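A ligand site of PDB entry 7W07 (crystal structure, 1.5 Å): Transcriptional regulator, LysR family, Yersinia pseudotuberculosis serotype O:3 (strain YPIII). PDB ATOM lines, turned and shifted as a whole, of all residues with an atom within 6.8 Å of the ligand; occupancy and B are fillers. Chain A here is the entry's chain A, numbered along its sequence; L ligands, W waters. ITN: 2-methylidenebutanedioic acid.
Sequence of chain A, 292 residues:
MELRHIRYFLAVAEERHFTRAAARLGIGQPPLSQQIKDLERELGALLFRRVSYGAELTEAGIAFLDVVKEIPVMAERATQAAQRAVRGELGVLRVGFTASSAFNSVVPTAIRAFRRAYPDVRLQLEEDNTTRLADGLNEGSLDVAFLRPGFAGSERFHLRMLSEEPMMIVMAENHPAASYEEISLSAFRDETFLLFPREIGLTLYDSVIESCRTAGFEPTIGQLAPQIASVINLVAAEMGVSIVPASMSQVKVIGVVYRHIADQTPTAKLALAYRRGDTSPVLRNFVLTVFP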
ATOM      1  N   THR A  98      18.777   6.374   8.474  1.00  0.00           N
ATOM      2  CA  THR A  98      17.728   6.058   7.512  1.00  0.00           C
ATOM      3  C   THR A  98      16.866   7.282   7.232  1.00  0.00           C
ATOM      4  O   THR A  98      16.786   8.201   8.041  1.00  0.00           O
ATOM      5  CB  THR A  98      16.823   4.901   7.958  1.00  0.00           C
ATOM      6  OG1 THR A  98      15.838   5.393   8.891  1.00  0.00           O
ATOM      7  CG2 THR A  98      17.634   3.753   8.596  1.00  0.00           C
ATOM      8  N   ALA A  99      16.192   7.260   6.079  1.00  0.00           N
ATOM      9  CA  ALA A  99      15.408   8.440   5.709  1.00  0.00           C
ATOM     10  C   ALA A  99      14.330   8.753   6.750  1.00  0.00           C
ATOM     11  O   ALA A  99      14.106   9.911   7.096  1.00  0.00           O
ATOM     12  CB  ALA A  99      14.789   8.277   4.323  1.00  0.00           C
ATOM     13  N   SER A 100      13.641   7.723   7.257  1.00  0.00           N
ATOM     14  CA  SER A 100      12.624   8.004   8.254  1.00  0.00           C
ATOM     15  C   SER A 100      13.237   8.418   9.581  1.00  0.00           C
ATOM     16  O   SER A 100      12.640   9.232  10.292  1.00  0.00           O
ATOM     17  CB  SER A 100      11.651   6.833   8.454  1.00  0.00           C
ATOM     18  OG  SER A 100      12.334   5.679   8.941  1.00  0.00           O
ATOM     19  N   SER A 101      14.418   7.878   9.921  1.00  0.00           N
ATOM     20  CA  SER A 101      15.031   8.180  11.204  1.00  0.00           C
ATOM     21  C   SER A 101      15.350   9.658  11.353  1.00  0.00           C
ATOM     22  O   SER A 101      15.397  10.164  12.470  1.00  0.00           O
ATOM     23  CB  SER A 101      16.275   7.333  11.427  1.00  0.00           C
ATOM     24  OG  SER A 101      17.369   7.828  10.685  1.00  0.00           O
ATOM     25  N   ASP A 128      20.529   6.291   4.104  1.00  0.00           N
ATOM     26  CA  ASP A 128      20.268   5.003   3.471  1.00  0.00           C
ATOM     27  C   ASP A 128      19.656   4.081   4.505  1.00  0.00           C
ATOM     28  O   ASP A 128      19.659   4.360   5.708  1.00  0.00           O
ATOM     29  CB  ASP A 128      21.552   4.393   2.885  1.00  0.00           C
ATOM     30  CG  ASP A 128      21.304   3.698   1.536  1.00  0.00           C
ATOM     31  OD1 ASP A 128      20.231   3.083   1.303  1.00  0.00           O
ATOM     32  OD2 ASP A 128      22.241   3.775   0.701  1.00  0.00           O
ATOM     33  N   ASN A 129      19.121   2.970   4.005  1.00  0.00           N
ATOM     34  CA  ASN A 129      18.366   2.066   4.856  1.00  0.00           C
ATOM     35  C   ASN A 129      19.303   1.174   5.641  1.00  0.00           C
ATOM     36  O   ASN A 129      20.502   1.087   5.368  1.00  0.00           O
ATOM     37  CB  ASN A 129      17.402   1.267   3.997  1.00  0.00           C
ATOM     38  CG  ASN A 129      16.416   2.146   3.307  1.00  0.00           C
ATOM     39  OD1 ASN A 129      16.568   2.486   2.133  1.00  0.00           O
ATOM     40  ND2 ASN A 129      15.401   2.584   4.057  1.00  0.00           N
ATOM     41  N   THR A 130      18.722   0.490   6.643  1.00  0.00           N
ATOM     42  CA  THR A 130      19.511  -0.281   7.603  1.00  0.00           C
ATOM     43  C   THR A 130      20.404  -1.310   6.930  1.00  0.00           C
ATOM     44  O   THR A 130      21.564  -1.464   7.315  1.00  0.00           O
ATOM     45  CB  THR A 130      18.593  -0.940   8.639  1.00  0.00           C
ATOM     46  OG1 THR A 130      18.008   0.076   9.462  1.00  0.00           O
ATOM     47  CG2 THR A 130      19.371  -1.938   9.537  1.00  0.00           C
ATOM     48  N   THR A 131      19.896  -2.023   5.919  1.00  0.00           N
ATOM     49  CA  THR A 131      20.743  -2.995   5.238  1.00  0.00           C
ATOM     50  C   THR A 131      22.018  -2.345   4.713  1.00  0.00           C
ATOM     51  O   THR A 131      23.126  -2.833   4.964  1.00  0.00           O
ATOM     52  CB  THR A 131      19.966  -3.672   4.113  1.00  0.00           C
ATOM     53  OG1 THR A 131      18.842  -4.358   4.677  1.00  0.00           O
ATOM     54  CG2 THR A 131      20.866  -4.646   3.364  1.00  0.00           C
ATOM     55  N   LEU A 133      23.303   0.648   5.574  1.00  0.00           N
ATOM     56  CA  LEU A 133      24.094   1.241   6.645  1.00  0.00           C
ATOM     57  C   LEU A 133      24.963   0.187   7.332  1.00  0.00           C
ATOM     58  O   LEU A 133      26.135   0.421   7.613  1.00  0.00           O
ATOM     59  CB  LEU A 133      23.181   1.928   7.662  1.00  0.00           C
ATOM     60  CG  LEU A 133      22.372   3.137   7.154  1.00  0.00           C
ATOM     61  CD1 LEU A 133      21.396   3.648   8.213  1.00  0.00           C
ATOM     62  CD2 LEU A 133      23.279   4.267   6.677  1.00  0.00           C
ATOM     63  N   LEU A 147      20.406   3.436  12.943  1.00  0.00           N
ATOM     64  CA  LEU A 147      19.767   2.375  12.175  1.00  0.00           C
ATOM     65  C   LEU A 147      18.789   1.621  13.051  1.00  0.00           C
ATOM     66  O   LEU A 147      18.655   1.864  14.255  1.00  0.00           O
ATOM     67  CB  LEU A 147      20.798   1.466  11.492  1.00  0.00           C
ATOM     68  CG  LEU A 147      21.942   0.869  12.324  1.00  0.00           C
ATOM     69  CD1 LEU A 147      21.435  -0.129  13.370  1.00  0.00           C
ATOM     70  CD2 LEU A 147      22.889   0.182  11.360  1.00  0.00           C
ATOM     71  N   ARG A 148      18.098   0.661  12.458  1.00  0.00           N
ATOM     72  CA  ARG A 148      17.115  -0.077  13.217  1.00  0.00           C
ATOM     73  C   ARG A 148      17.741  -1.375  13.696  1.00  0.00           C
ATOM     74  O   ARG A 148      18.281  -2.136  12.878  1.00  0.00           O
ATOM     75  CB  ARG A 148      15.886  -0.322  12.350  1.00  0.00           C
ATOM     76  CG  ARG A 148      15.389   1.018  11.786  1.00  0.00           C
ATOM     77  CD  ARG A 148      13.890   1.048  11.583  1.00  0.00           C
ATOM     78  NE  ARG A 148      13.460   2.402  11.219  1.00  0.00           N
ATOM     79  CZ  ARG A 148      13.106   3.348  12.071  1.00  0.00           C
ATOM     80  NH1 ARG A 148      13.149   3.127  13.390  1.00  0.00           N
ATOM     81  NH2 ARG A 148      12.728   4.540  11.626  1.00  0.00           N
ATOM     82  N   PHE A 196       7.584  -0.406   1.822  1.00  0.00           N
ATOM     83  CA  PHE A 196       8.862  -0.342   1.123  1.00  0.00           C
ATOM     84  C   PHE A 196       9.394  -1.762   0.931  1.00  0.00           C
ATOM     85  O   PHE A 196       8.958  -2.691   1.610  1.00  0.00           O
ATOM     86  CB  PHE A 196       9.848   0.465   1.964  1.00  0.00           C
ATOM     87  CG  PHE A 196       9.960  -0.017   3.390  1.00  0.00           C
ATOM     88  CD1 PHE A 196      10.845  -1.022   3.737  1.00  0.00           C
ATOM     89  CD2 PHE A 196       9.162   0.549   4.380  1.00  0.00           C
ATOM     90  CE1 PHE A 196      10.928  -1.459   5.042  1.00  0.00           C
ATOM     91  CE2 PHE A 196       9.259   0.114   5.681  1.00  0.00           C
ATOM     92  CZ  PHE A 196      10.130  -0.894   6.010  1.00  0.00           C
ATOM     93  N   PRO A 197      10.334  -1.961   0.003  1.00  0.00           N
ATOM     94  CA  PRO A 197      10.837  -3.322  -0.238  1.00  0.00           C
ATOM     95  C   PRO A 197      11.551  -3.875   0.987  1.00  0.00           C
ATOM     96  O   PRO A 197      12.420  -3.231   1.570  1.00  0.00           O
ATOM     97  CB  PRO A 197      11.807  -3.136  -1.413  1.00  0.00           C
ATOM     98  CG  PRO A 197      11.394  -1.832  -2.045  1.00  0.00           C
ATOM     99  CD  PRO A 197      10.927  -0.975  -0.915  1.00  0.00           C
ATOM    100  N   ILE A 200      15.533  -3.748   2.095  1.00  0.00           N
ATOM    101  CA  ILE A 200      16.256  -2.576   2.581  1.00  0.00           C
ATOM    102  C   ILE A 200      16.232  -2.450   4.097  1.00  0.00           C
ATOM    103  O   ILE A 200      17.057  -1.724   4.667  1.00  0.00           O
ATOM    104  CB  ILE A 200      15.738  -1.271   1.936  1.00  0.00           C
ATOM    105  CG1 ILE A 200      14.432  -0.806   2.590  1.00  0.00           C
ATOM    106  CG2 ILE A 200      15.557  -1.457   0.453  1.00  0.00           C
ATOM    107  CD1 ILE A 200      13.807   0.415   1.875  1.00  0.00           C
ATOM    108  N   GLY A 201      15.305  -3.118   4.776  1.00  0.00           N
ATOM    109  CA  GLY A 201      15.114  -2.969   6.199  1.00  0.00           C
ATOM    110  C   GLY A 201      14.230  -4.091   6.703  1.00  0.00           C
ATOM    111  O   GLY A 201      13.013  -3.930   6.860  1.00  0.00           O
ATOM    112  N   LEU A 202      14.832  -5.262   6.927  1.00  0.00           N
ATOM    113  CA  LEU A 202      14.043  -6.455   7.202  1.00  0.00           C
ATOM    114  C   LEU A 202      13.280  -6.322   8.510  1.00  0.00           C
ATOM    115  O   LEU A 202      12.124  -6.751   8.613  1.00  0.00           O
ATOM    116  CB  LEU A 202      14.944  -7.685   7.240  1.00  0.00           C
ATOM    117  CG  LEU A 202      15.305  -8.329   5.892  1.00  0.00           C
ATOM    118  CD1 LEU A 202      16.247  -7.450   5.079  1.00  0.00           C
ATOM    119  CD2 LEU A 202      15.907  -9.711   6.120  1.00  0.00           C
ATOM    120  N   THR A 203      13.923  -5.757   9.533  1.00  0.00           N
ATOM    121  CA  THR A 203      13.322  -5.730  10.866  1.00  0.00           C
ATOM    122  C   THR A 203      12.066  -4.872  10.876  1.00  0.00           C
ATOM    123  O   THR A 203      11.002  -5.329  11.336  1.00  0.00           O
ATOM    124  CB  THR A 203      14.328  -5.221  11.891  1.00  0.00           C
ATOM    125  OG1 THR A 203      15.385  -6.180  12.013  1.00  0.00           O
ATOM    126  CG2 THR A 203      13.660  -5.058  13.224  1.00  0.00           C
ATOM    127  N   LEU A 204      12.146  -3.644  10.365  1.00  0.00           N
ATOM    128  CA  LEU A 204      10.963  -2.791  10.342  1.00  0.00           C
ATOM    129  C   LEU A 204       9.872  -3.386   9.461  1.00  0.00           C
ATOM    130  O   LEU A 204       8.700  -3.417   9.846  1.00  0.00           O
ATOM    131  CB  LEU A 204      11.320  -1.369   9.887  1.00  0.00           C
ATOM    132  CG  LEU A 204      10.133  -0.425  10.017  1.00  0.00           C
ATOM    133  CD1 LEU A 204       9.709  -0.278  11.492  1.00  0.00           C
ATOM    134  CD2 LEU A 204      10.454   0.936   9.401  1.00  0.00           C
ATOM    135  N   TYR A 205      10.239  -3.872   8.269  1.00  0.00           N
ATOM    136  CA  TYR A 205       9.253  -4.519   7.396  1.00  0.00           C
ATOM    137  C   TYR A 205       8.557  -5.666   8.118  1.00  0.00           C
ATOM    138  O   TYR A 205       7.326  -5.743   8.154  1.00  0.00           O
ATOM    139  CB  TYR A 205       9.939  -4.993   6.121  1.00  0.00           C
ATOM    140  CG  TYR A 205       9.017  -5.613   5.095  1.00  0.00           C
ATOM    141  CD1 TYR A 205       8.574  -6.923   5.238  1.00  0.00           C
ATOM    142  CD2 TYR A 205       8.614  -4.903   3.980  1.00  0.00           C
ATOM    143  CE1 TYR A 205       7.738  -7.495   4.292  1.00  0.00           C
ATOM    144  CE2 TYR A 205       7.774  -5.472   3.025  1.00  0.00           C
ATOM    145  CZ  TYR A 205       7.336  -6.761   3.195  1.00  0.00           C
ATOM    146  OH  TYR A 205       6.505  -7.348   2.254  1.00  0.00           O
ATOM    147  N   PRO A 226       9.876   3.292  -2.617  1.00  0.00           N
ATOM    148  CA  PRO A 226      11.254   3.116  -2.127  1.00  0.00           C
ATOM    149  C   PRO A 226      11.470   3.426  -0.666  1.00  0.00           C
ATOM    150  O   PRO A 226      12.284   2.759  -0.011  1.00  0.00           O
ATOM    151  CB  PRO A 226      12.063   4.042  -3.051  1.00  0.00           C
ATOM    152  CG  PRO A 226      11.250   4.072  -4.310  1.00  0.00           C
ATOM    153  CD  PRO A 226       9.825   4.127  -3.829  1.00  0.00           C
ATOM    154  N   GLN A 227      10.809   4.471  -0.174  1.00  0.00           N
ATOM    155  CA  GLN A 227      10.981   4.911   1.220  1.00  0.00           C
ATOM    156  C   GLN A 227       9.622   5.130   1.879  1.00  0.00           C
ATOM    157  O   GLN A 227       8.655   5.202   1.211  1.00  0.00           O
ATOM    158  CB  GLN A 227      11.822   6.180   1.293  1.00  0.00           C
ATOM    159  CG  GLN A 227      13.217   6.047   0.701  1.00  0.00           C
ATOM    160  CD  GLN A 227      14.117   5.095   1.450  1.00  0.00           C
ATOM    161  OE1 GLN A 227      13.964   4.905   2.623  1.00  0.00           O
ATOM    162  NE2 GLN A 227      15.053   4.504   0.754  1.00  0.00           N
ATOM    163  N   ILE A 228       9.615   5.304   3.189  1.00  0.00           N
ATOM    164  CA  ILE A 228       8.326   5.497   3.879  1.00  0.00           C
ATOM    165  C   ILE A 228       7.682   6.796   3.419  1.00  0.00           C
ATOM    166  O   ILE A 228       6.529   6.834   3.244  1.00  0.00           O
ATOM    167  CB  ILE A 228       8.526   5.422   5.389  1.00  0.00           C
ATOM    168  CG1 ILE A 228       8.969   4.009   5.798  1.00  0.00           C
ATOM    169  CG2 ILE A 228       7.258   5.847   6.106  1.00  0.00           C
ATOM    170  CD1 ILE A 228       9.418   3.949   7.243  1.00  0.00           C
ATOM    171  N   PRO A 245       6.634   4.628  11.644  1.00  0.00           N
ATOM    172  CA  PRO A 245       7.073   5.207  12.923  1.00  0.00           C
ATOM    173  C   PRO A 245       6.290   6.488  13.211  1.00  0.00           C
ATOM    174  O   PRO A 245       6.022   7.274  12.309  1.00  0.00           O
ATOM    175  CB  PRO A 245       8.567   5.500  12.697  1.00  0.00           C
ATOM    176  CG  PRO A 245       8.981   4.532  11.611  1.00  0.00           C
ATOM    177  CD  PRO A 245       7.753   4.410  10.713  1.00  0.00           C
ATOM    178  N   MET A 248       6.882   9.900  11.711  1.00  0.00           N
ATOM    179  CA  MET A 248       6.500  10.209  10.345  1.00  0.00           C
ATOM    180  C   MET A 248       5.174  10.944  10.257  1.00  0.00           C
ATOM    181  O   MET A 248       4.813  11.400   9.173  1.00  0.00           O
ATOM    182  CB  MET A 248       6.514   8.966   9.456  1.00  0.00           C
ATOM    183  CG  MET A 248       7.889   8.318   9.369  1.00  0.00           C
ATOM    184  SD  MET A 248       9.108   9.429   8.612  1.00  0.00           S
ATOM    185  CE  MET A 248       8.557   9.512   6.890  1.00  0.00           C
ATOM    186  N   LEU A 270      15.237   2.761  17.063  1.00  0.00           N
ATOM    187  CA  LEU A 270      16.411   3.409  16.490  1.00  0.00           C
ATOM    188  C   LEU A 270      17.585   3.238  17.447  1.00  0.00           C
ATOM    189  O   LEU A 270      17.472   3.563  18.633  1.00  0.00           O
ATOM    190  CB  LEU A 270      16.140   4.896  16.246  1.00  0.00           C
ATOM    191  CG  LEU A 270      17.071   5.609  15.277  1.00  0.00           C
ATOM    192  CD1 LEU A 270      17.036   4.932  13.913  1.00  0.00           C
ATOM    193  CD2 LEU A 270      16.687   7.092  15.167  1.00  0.00           C
HETATM  194  C1  ITN L   1      15.134   0.707   7.548  1.00  0.00           C
HETATM  195  C2  ITN L   1      13.629   0.729   7.323  1.00  0.00           C
HETATM  196  C3  ITN L   1      13.192   2.037   6.691  1.00  0.00           C
HETATM  197  C5  ITN L   1      13.513   3.331   7.412  1.00  0.00           C
HETATM  198  O3  ITN L   1      13.985   3.290   8.585  1.00  0.00           O
HETATM  199  O4  ITN L   1      13.267   4.425   6.828  1.00  0.00           O
HETATM  200  C4  ITN L   1      12.481   2.017   5.565  1.00  0.00           C
HETATM  201  O1  ITN L   1      15.913   1.309   6.755  1.00  0.00           O
HETATM  202  O2  ITN L   1      15.577   0.091   8.551  1.00  0.00           O
HETATM  203  O   HOH W   1      12.164   5.553   4.622  1.00  0.00           O
HETATM  204  O   HOH W   2      14.629  -2.395   9.441  1.00  0.00           O
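An oxygen (O1) of the ligand lies within hydrogen-bond range of the backbone NH (N) of Thr 130 (2.9 Å). The side-chain hydroxyl (OG1) of Thr 98 sits at hydrogen-bond distance from an oxygen (O3) of the ligand (2.8 Å). O4 of the ligand sits close to N of Ser 100. An oxygen (O1) of the ligand sits at hydrogen-bond distance from the side-chain amide nitrogen of Asn 129. The side-chain hydroxyl of Ser 100 sits at hydrogen-bond distance from an oxygen (O4) of the ligand, 2.6 Å away. The guanidinium group (NE) of Arg 148 is in salt-bridge range of an oxygen (O3) of the ligand (2.8 Å). OG1 of Thr 130 sits at hydrogen-bond distance from O2 of the ligand, 2.6 Å away.
The side-chain hydroxyl of Ser 101 sits at hydrogen-bond distance from the backbone carbonyl oxygen of Thr 98. The side-chain hydroxyl (OG) of Ser 100 sits at hydrogen-bond distance from the guanidinium group (NH2) of Arg 148 (2.9 Å). The backbone carbonyl oxygen of Ile 200 is in hydrogen-bond range of the backbone NH of Thr 130 (3.4 Å). The side-chain amide nitrogen (NE2) of Gln 227 is in hydrogen-bond range of the side-chain amide oxygen (OD1) of Asn 129 (2.9 Å). O of Ile 200 is in hydrogen-bond range of N of Thr 131, at 3.1 Å. The backbone NH (N) of Arg 148 is in hydrogen-bond range of the side-chain hydroxyl (OG1) of Thr 130, 3.1 Å away.
Phe 196 touches the ligand. O of Ile 200 touches O1 of the ligand, at 3.9 Å. Gly 201 touches the ligand. CD2 of Leu 204 touches C2 of the ligand, at 3.8 Å. Ile 228 touches the ligand. Hydrophobic or aromatic side chains within 4 Å of the ligand: Phe 196, Leu 204 and Ile 228. Ten residues have an atom within 4 Å of the ligand: Thr 98, Ser 100, Asn 129, Thr 130, Arg 148, Phe 196, Ile 200, Gly 201, Leu 204 and Ile 228. The nearest printed residue that does not touch the ligand is Ala 99 (4.1 Å).
Water W1 lies within hydrogen-bond range of an oxygen (O4) of the ligand (2.7 Å), the side-chain amide oxygen of Gln 227 (2.8 Å) and the backbone NH of Ile 228 (2.9 Å). Water W2 lies within hydrogen-bond range of O2 of the ligand (2.8 Å), N of Leu 204 (2.9 Å), O of Gly 201 (3.4 Å) and N of Thr 203 (3.4 Å).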
